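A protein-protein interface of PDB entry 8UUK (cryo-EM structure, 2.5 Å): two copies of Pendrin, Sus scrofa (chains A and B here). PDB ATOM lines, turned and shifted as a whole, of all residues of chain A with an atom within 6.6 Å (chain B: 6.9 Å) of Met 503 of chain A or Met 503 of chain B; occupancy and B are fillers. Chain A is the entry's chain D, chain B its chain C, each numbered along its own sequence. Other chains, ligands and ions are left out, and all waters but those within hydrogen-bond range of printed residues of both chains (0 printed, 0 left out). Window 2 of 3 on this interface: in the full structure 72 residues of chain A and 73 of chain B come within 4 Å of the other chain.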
ATOM      1  N   LEU A 219     -12.364   8.087  16.616  1.00  0.00           N
ATOM      2  CA  LEU A 219     -11.509   7.775  17.755  1.00  0.00           C
ATOM      3  C   LEU A 219     -11.391   6.273  17.955  1.00  0.00           C
ATOM      4  O   LEU A 219     -10.333   5.790  18.366  1.00  0.00           O
ATOM      5  CB  LEU A 219     -12.021   8.464  19.023  1.00  0.00           C
ATOM      6  CG  LEU A 219     -13.100   7.861  19.923  1.00  0.00           C
ATOM      7  CD1 LEU A 219     -12.493   6.980  21.003  1.00  0.00           C
ATOM      8  CD2 LEU A 219     -13.911   8.976  20.556  1.00  0.00           C
ATOM      9  N   PHE A 484      -5.482  12.263  16.712  1.00  0.00           N
ATOM     10  CA  PHE A 484      -5.209  12.543  18.115  1.00  0.00           C
ATOM     11  C   PHE A 484      -5.358  11.290  18.961  1.00  0.00           C
ATOM     12  O   PHE A 484      -4.534  11.035  19.843  1.00  0.00           O
ATOM     13  CB  PHE A 484      -6.133  13.644  18.634  1.00  0.00           C
ATOM     14  CG  PHE A 484      -5.875  14.017  20.068  1.00  0.00           C
ATOM     15  CD1 PHE A 484      -4.956  15.000  20.383  1.00  0.00           C
ATOM     16  CD2 PHE A 484      -6.545  13.380  21.098  1.00  0.00           C
ATOM     17  CE1 PHE A 484      -4.712  15.343  21.697  1.00  0.00           C
ATOM     18  CE2 PHE A 484      -6.302  13.718  22.413  1.00  0.00           C
ATOM     19  CZ  PHE A 484      -5.387  14.701  22.712  1.00  0.00           C
ATOM     20  N   LEU A 498      -7.296   6.089  25.433  1.00  0.00           N
ATOM     21  CA  LEU A 498      -8.743   6.064  25.246  1.00  0.00           C
ATOM     22  C   LEU A 498      -9.411   7.222  25.970  1.00  0.00           C
ATOM     23  O   LEU A 498     -10.313   7.871  25.424  1.00  0.00           O
ATOM     24  CB  LEU A 498      -9.319   4.740  25.742  1.00  0.00           C
ATOM     25  CG  LEU A 498     -10.837   4.635  25.580  1.00  0.00           C
ATOM     26  CD1 LEU A 498     -11.198   4.109  24.200  1.00  0.00           C
ATOM     27  CD2 LEU A 498     -11.461   3.794  26.680  1.00  0.00           C
ATOM     28  N   LEU A 499      -8.994   7.484  27.212  1.00  0.00           N
ATOM     29  CA  LEU A 499      -9.576   8.596  27.955  1.00  0.00           C
ATOM     30  C   LEU A 499      -9.304   9.923  27.257  1.00  0.00           C
ATOM     31  O   LEU A 499     -10.201  10.762  27.135  1.00  0.00           O
ATOM     32  CB  LEU A 499      -9.038   8.618  29.386  1.00  0.00           C
ATOM     33  CG  LEU A 499      -9.401   7.411  30.251  1.00  0.00           C
ATOM     34  CD1 LEU A 499      -8.895   7.599  31.670  1.00  0.00           C
ATOM     35  CD2 LEU A 499     -10.902   7.180  30.243  1.00  0.00           C
ATOM     36  N   ALA A 500      -8.075  10.117  26.772  1.00  0.00           N
ATOM     37  CA  ALA A 500      -7.735  11.345  26.064  1.00  0.00           C
ATOM     38  C   ALA A 500      -8.518  11.472  24.764  1.00  0.00           C
ATOM     39  O   ALA A 500      -8.935  12.570  24.391  1.00  0.00           O
ATOM     40  CB  ALA A 500      -6.232  11.394  25.793  1.00  0.00           C
ATOM     41  N   GLY A 501      -8.721  10.360  24.055  1.00  0.00           N
ATOM     42  CA  GLY A 501      -9.503  10.411  22.831  1.00  0.00           C
ATOM     43  C   GLY A 501     -10.955  10.772  23.078  1.00  0.00           C
ATOM     44  O   GLY A 501     -11.533  11.587  22.356  1.00  0.00           O
ATOM     45  N   LEU A 502     -11.562  10.176  24.107  1.00  0.00           N
ATOM     46  CA  LEU A 502     -12.924  10.547  24.488  1.00  0.00           C
ATOM     47  C   LEU A 502     -13.005  12.018  24.870  1.00  0.00           C
ATOM     48  O   LEU A 502     -13.926  12.742  24.460  1.00  0.00           O
ATOM     49  CB  LEU A 502     -13.395   9.678  25.652  1.00  0.00           C
ATOM     50  CG  LEU A 502     -13.956   8.302  25.325  1.00  0.00           C
ATOM     51  CD1 LEU A 502     -13.978   7.444  26.570  1.00  0.00           C
ATOM     52  CD2 LEU A 502     -15.347   8.446  24.750  1.00  0.00           C
ATOM     53  N   MET A 503     -12.031  12.479  25.653  1.00  0.00           N
ATOM     54  CA  MET A 503     -12.014  13.851  26.116  1.00  0.00           C
ATOM     55  C   MET A 503     -11.866  14.819  24.953  1.00  0.00           C
ATOM     56  O   MET A 503     -12.533  15.860  24.926  1.00  0.00           O
ATOM     57  CB  MET A 503     -10.851  14.035  27.081  1.00  0.00           C
ATOM     58  CG  MET A 503     -11.084  13.434  28.451  1.00  0.00           C
ATOM     59  SD  MET A 503     -12.636  13.849  29.239  1.00  0.00           S
ATOM     60  CE  MET A 503     -13.327  12.228  29.540  1.00  0.00           C
ATOM     61  N   PHE A 504     -11.025  14.467  23.979  1.00  0.00           N
ATOM     62  CA  PHE A 504     -10.834  15.284  22.789  1.00  0.00           C
ATOM     63  C   PHE A 504     -12.074  15.274  21.907  1.00  0.00           C
ATOM     64  O   PHE A 504     -12.377  16.273  21.254  1.00  0.00           O
ATOM     65  CB  PHE A 504      -9.613  14.790  22.012  1.00  0.00           C
ATOM     66  CG  PHE A 504      -9.173  15.718  20.915  1.00  0.00           C
ATOM     67  CD1 PHE A 504      -8.460  16.867  21.208  1.00  0.00           C
ATOM     68  CD2 PHE A 504      -9.469  15.441  19.596  1.00  0.00           C
ATOM     69  CE1 PHE A 504      -8.056  17.714  20.210  1.00  0.00           C
ATOM     70  CE2 PHE A 504      -9.068  16.288  18.595  1.00  0.00           C
ATOM     71  CZ  PHE A 504      -8.363  17.423  18.898  1.00  0.00           C
ATOM     72  N   GLY A 505     -12.801  14.156  21.861  1.00  0.00           N
ATOM     73  CA  GLY A 505     -14.076  14.158  21.161  1.00  0.00           C
ATOM     74  C   GLY A 505     -15.070  15.120  21.782  1.00  0.00           C
ATOM     75  O   GLY A 505     -15.746  15.878  21.078  1.00  0.00           O
ATOM     76  N   PHE A 506     -15.159  15.111  23.115  1.00  0.00           N
ATOM     77  CA  PHE A 506     -16.009  16.083  23.798  1.00  0.00           C
ATOM     78  C   PHE A 506     -15.558  17.508  23.500  1.00  0.00           C
ATOM     79  O   PHE A 506     -16.384  18.394  23.245  1.00  0.00           O
ATOM     80  CB  PHE A 506     -15.994  15.832  25.305  1.00  0.00           C
ATOM     81  CG  PHE A 506     -16.613  14.531  25.712  1.00  0.00           C
ATOM     82  CD1 PHE A 506     -17.546  13.909  24.904  1.00  0.00           C
ATOM     83  CD2 PHE A 506     -16.270  13.934  26.911  1.00  0.00           C
ATOM     84  CE1 PHE A 506     -18.116  12.716  25.280  1.00  0.00           C
ATOM     85  CE2 PHE A 506     -16.840  12.738  27.293  1.00  0.00           C
ATOM     86  CZ  PHE A 506     -17.765  12.129  26.476  1.00  0.00           C
ATOM     87  N   LEU A 507     -14.245  17.744  23.520  1.00  0.00           N
ATOM     88  CA  LEU A 507     -13.721  19.078  23.250  1.00  0.00           C
ATOM     89  C   LEU A 507     -14.030  19.520  21.824  1.00  0.00           C
ATOM     90  O   LEU A 507     -14.339  20.691  21.585  1.00  0.00           O
ATOM     91  CB  LEU A 507     -12.215  19.109  23.505  1.00  0.00           C
ATOM     92  CG  LEU A 507     -11.509  20.438  23.243  1.00  0.00           C
ATOM     93  CD1 LEU A 507     -11.833  21.443  24.338  1.00  0.00           C
ATOM     94  CD2 LEU A 507     -10.008  20.236  23.113  1.00  0.00           C
ATOM     95  N   THR A 508     -13.942  18.602  20.861  1.00  0.00           N
ATOM     96  CA  THR A 508     -14.260  18.941  19.478  1.00  0.00           C
ATOM     97  C   THR A 508     -15.737  19.259  19.311  1.00  0.00           C
ATOM     98  O   THR A 508     -16.096  20.175  18.563  1.00  0.00           O
ATOM     99  CB  THR A 508     -13.852  17.804  18.543  1.00  0.00           C
ATOM    100  OG1 THR A 508     -14.373  16.564  19.036  1.00  0.00           O
ATOM    101  CG2 THR A 508     -12.341  17.719  18.433  1.00  0.00           C
ATOM    102  N   LEU B 219     -19.254  27.636  37.097  1.00  0.00           N
ATOM    103  CA  LEU B 219     -18.057  26.964  37.587  1.00  0.00           C
ATOM    104  C   LEU B 219     -17.103  27.953  38.237  1.00  0.00           C
ATOM    105  O   LEU B 219     -16.424  27.603  39.207  1.00  0.00           O
ATOM    106  CB  LEU B 219     -17.367  26.191  36.459  1.00  0.00           C
ATOM    107  CG  LEU B 219     -16.370  26.833  35.494  1.00  0.00           C
ATOM    108  CD1 LEU B 219     -14.949  26.740  36.026  1.00  0.00           C
ATOM    109  CD2 LEU B 219     -16.467  26.157  34.141  1.00  0.00           C
ATOM    110  N   PHE B 484     -20.799  20.904  41.233  1.00  0.00           N
ATOM    111  CA  PHE B 484     -19.726  19.979  40.898  1.00  0.00           C
ATOM    112  C   PHE B 484     -18.368  20.653  41.011  1.00  0.00           C
ATOM    113  O   PHE B 484     -17.421  20.061  41.532  1.00  0.00           O
ATOM    114  CB  PHE B 484     -19.920  19.415  39.493  1.00  0.00           C
ATOM    115  CG  PHE B 484     -18.870  18.415  39.095  1.00  0.00           C
ATOM    116  CD1 PHE B 484     -19.035  17.072  39.379  1.00  0.00           C
ATOM    117  CD2 PHE B 484     -17.716  18.819  38.446  1.00  0.00           C
ATOM    118  CE1 PHE B 484     -18.072  16.151  39.020  1.00  0.00           C
ATOM    119  CE2 PHE B 484     -16.749  17.903  38.089  1.00  0.00           C
ATOM    120  CZ  PHE B 484     -16.928  16.568  38.374  1.00  0.00           C
ATOM    121  N   LEU B 498     -10.310  22.850  39.373  1.00  0.00           N
ATOM    122  CA  LEU B 498     -10.564  23.709  38.220  1.00  0.00           C
ATOM    123  C   LEU B 498     -10.611  22.904  36.930  1.00  0.00           C
ATOM    124  O   LEU B 498     -11.488  23.122  36.086  1.00  0.00           O
ATOM    125  CB  LEU B 498      -9.492  24.791  38.116  1.00  0.00           C
ATOM    126  CG  LEU B 498      -9.682  25.734  36.928  1.00  0.00           C
ATOM    127  CD1 LEU B 498     -10.595  26.890  37.300  1.00  0.00           C
ATOM    128  CD2 LEU B 498      -8.351  26.231  36.394  1.00  0.00           C
ATOM    129  N   LEU B 499      -9.664  21.981  36.751  1.00  0.00           N
ATOM    130  CA  LEU B 499      -9.662  21.162  35.541  1.00  0.00           C
ATOM    131  C   LEU B 499     -10.922  20.311  35.456  1.00  0.00           C
ATOM    132  O   LEU B 499     -11.542  20.198  34.388  1.00  0.00           O
ATOM    133  CB  LEU B 499      -8.418  20.279  35.512  1.00  0.00           C
ATOM    134  CG  LEU B 499      -7.089  21.029  35.448  1.00  0.00           C
ATOM    135  CD1 LEU B 499      -5.929  20.058  35.337  1.00  0.00           C
ATOM    136  CD2 LEU B 499      -7.087  22.011  34.293  1.00  0.00           C
ATOM    137  N   ALA B 500     -11.321  19.711  36.580  1.00  0.00           N
ATOM    138  CA  ALA B 500     -12.527  18.896  36.605  1.00  0.00           C
ATOM    139  C   ALA B 500     -13.762  19.732  36.304  1.00  0.00           C
ATOM    140  O   ALA B 500     -14.650  19.287  35.574  1.00  0.00           O
ATOM    141  CB  ALA B 500     -12.666  18.201  37.957  1.00  0.00           C
ATOM    142  N   GLY B 501     -13.837  20.945  36.853  1.00  0.00           N
ATOM    143  CA  GLY B 501     -14.970  21.806  36.561  1.00  0.00           C
ATOM    144  C   GLY B 501     -15.023  22.233  35.106  1.00  0.00           C
ATOM    145  O   GLY B 501     -16.096  22.272  34.500  1.00  0.00           O
ATOM    146  N   LEU B 502     -13.864  22.560  34.528  1.00  0.00           N
ATOM    147  CA  LEU B 502     -13.815  22.935  33.119  1.00  0.00           C
ATOM    148  C   LEU B 502     -14.306  21.801  32.235  1.00  0.00           C
ATOM    149  O   LEU B 502     -15.163  21.997  31.359  1.00  0.00           O
ATOM    150  CB  LEU B 502     -12.391  23.328  32.728  1.00  0.00           C
ATOM    151  CG  LEU B 502     -11.976  24.780  32.938  1.00  0.00           C
ATOM    152  CD1 LEU B 502     -10.470  24.906  32.842  1.00  0.00           C
ATOM    153  CD2 LEU B 502     -12.649  25.664  31.907  1.00  0.00           C
ATOM    154  N   MET B 503     -13.790  20.590  32.456  1.00  0.00           N
ATOM    155  CA  MET B 503     -14.236  19.514  31.585  1.00  0.00           C
ATOM    156  C   MET B 503     -15.647  19.057  31.927  1.00  0.00           C
ATOM    157  O   MET B 503     -16.324  18.473  31.079  1.00  0.00           O
ATOM    158  CB  MET B 503     -13.288  18.325  31.602  1.00  0.00           C
ATOM    159  CG  MET B 503     -12.265  18.364  30.484  1.00  0.00           C
ATOM    160  SD  MET B 503     -12.972  17.755  28.939  1.00  0.00           S
ATOM    161  CE  MET B 503     -14.220  16.627  29.553  1.00  0.00           C
ATOM    162  N   PHE B 504     -16.124  19.323  33.141  1.00  0.00           N
ATOM    163  CA  PHE B 504     -17.522  19.038  33.430  1.00  0.00           C
ATOM    164  C   PHE B 504     -18.430  20.008  32.690  1.00  0.00           C
ATOM    165  O   PHE B 504     -19.509  19.627  32.235  1.00  0.00           O
ATOM    166  CB  PHE B 504     -17.780  19.093  34.932  1.00  0.00           C
ATOM    167  CG  PHE B 504     -19.130  18.572  35.326  1.00  0.00           C
ATOM    168  CD1 PHE B 504     -19.367  17.210  35.397  1.00  0.00           C
ATOM    169  CD2 PHE B 504     -20.169  19.443  35.600  1.00  0.00           C
ATOM    170  CE1 PHE B 504     -20.602  16.730  35.758  1.00  0.00           C
ATOM    171  CE2 PHE B 504     -21.407  18.965  35.954  1.00  0.00           C
ATOM    172  CZ  PHE B 504     -21.623  17.608  36.034  1.00  0.00           C
ATOM    173  N   GLY B 505     -18.006  21.265  32.552  1.00  0.00           N
ATOM    174  CA  GLY B 505     -18.726  22.176  31.677  1.00  0.00           C
ATOM    175  C   GLY B 505     -18.744  21.691  30.241  1.00  0.00           C
ATOM    176  O   GLY B 505     -19.784  21.729  29.572  1.00  0.00           O
ATOM    177  N   PHE B 506     -17.598  21.209  29.753  1.00  0.00           N
ATOM    178  CA  PHE B 506     -17.561  20.623  28.413  1.00  0.00           C
ATOM    179  C   PHE B 506     -18.515  19.437  28.300  1.00  0.00           C
ATOM    180  O   PHE B 506     -19.245  19.306  27.309  1.00  0.00           O
ATOM    181  CB  PHE B 506     -16.141  20.182  28.057  1.00  0.00           C
ATOM    182  CG  PHE B 506     -15.158  21.307  27.952  1.00  0.00           C
ATOM    183  CD1 PHE B 506     -15.568  22.573  27.584  1.00  0.00           C
ATOM    184  CD2 PHE B 506     -13.813  21.088  28.190  1.00  0.00           C
ATOM    185  CE1 PHE B 506     -14.659  23.603  27.478  1.00  0.00           C
ATOM    186  CE2 PHE B 506     -12.899  22.115  28.084  1.00  0.00           C
ATOM    187  CZ  PHE B 506     -13.322  23.374  27.727  1.00  0.00           C
ATOM    188  N   LEU B 507     -18.520  18.563  29.306  1.00  0.00           N
ATOM    189  CA  LEU B 507     -19.392  17.395  29.287  1.00  0.00           C
ATOM    190  C   LEU B 507     -20.859  17.800  29.323  1.00  0.00           C
ATOM    191  O   LEU B 507     -21.696  17.173  28.669  1.00  0.00           O
ATOM    192  CB  LEU B 507     -19.055  16.472  30.457  1.00  0.00           C
ATOM    193  CG  LEU B 507     -19.863  15.177  30.557  1.00  0.00           C
ATOM    194  CD1 LEU B 507     -19.361  14.142  29.566  1.00  0.00           C
ATOM    195  CD2 LEU B 507     -19.812  14.632  31.974  1.00  0.00           C
ATOM    196  N   THR B 508     -21.193  18.839  30.089  1.00  0.00           N
ATOM    197  CA  THR B 508     -22.574  19.311  30.131  1.00  0.00           C
ATOM    198  C   THR B 508     -23.000  19.883  28.787  1.00  0.00           C
ATOM    199  O   THR B 508     -24.134  19.664  28.349  1.00  0.00           O
ATOM    200  CB  THR B 508     -22.754  20.352  31.235  1.00  0.00           C
ATOM    201  OG1 THR B 508     -21.741  21.358  31.122  1.00  0.00           O
ATOM    202  CG2 THR B 508     -22.673  19.699  32.605  1.00  0.00           C
ATOM    203  N   VAL B 509     -22.108  20.617  28.116  1.00  0.00           N
ATOM    204  CA  VAL B 509     -22.421  21.103  26.771  1.00  0.00           C
ATOM    205  C   VAL B 509     -22.658  19.933  25.825  1.00  0.00           C
ATOM    206  O   VAL B 509     -23.621  19.925  25.045  1.00  0.00           O
ATOM    207  CB  VAL B 509     -21.299  22.024  26.256  1.00  0.00           C
ATOM    208  CG1 VAL B 509     -21.550  22.402  24.806  1.00  0.00           C
ATOM    209  CG2 VAL B 509     -21.197  23.268  27.115  1.00  0.00           C
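Hydrophobic or aromatic side chains of chain A within 4 Å of the printed part of chain B: Met 503, Phe 506 and Leu 507.
Of the 14 printed residues of chain B, 3 touch a printed residue of chain A.
Among the printed residues, 3 pairs touch across the chains.
Among the printed residues, no Asp or Glu carboxylate lies within 4 Å of a Lys or Arg side-chain nitrogen of the other chain.
Among the printed residues, pairs that only touch across the chains: Met 503 of chain A with Met 503 of chain B (3.2 Å), Phe 506 of chain A with Leu 507 of chain B (3.7 Å) and Leu 507 of chain A with Phe 506 of chain B (3.95 Å).
Met 503 of chain A touches its own counterpart, Met 503 of chain B.
Phe 506 of chain A touches Leu 507 of chain B, and with the chains exchanged Leu 507 of chain A touches Phe 506 of chain B.
13 positions are printed for both chains.
Of the 3 pairs that touch across the chains among the printed residues, 3 have their exchanged pair printed and touching as well.
Met 503 of chain A touches just one residue of chain B: Met 503.
Printed residues of chain A within 4 Å of Leu 507 of chain B: Phe 506.
Of the printed residues of chain B, Phe 506 of chain A touches Leu 507 (3.7 Å).
Of the printed residues of chain B, Leu 507 of chain A touches Phe 506 (3.95 Å).
Leu 219 of chain B touches none of the printed residues of chain A.
The nearest residue of chain A that does not touch Met 503 of chain B is Phe 506 of chain A (4.3 Å).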
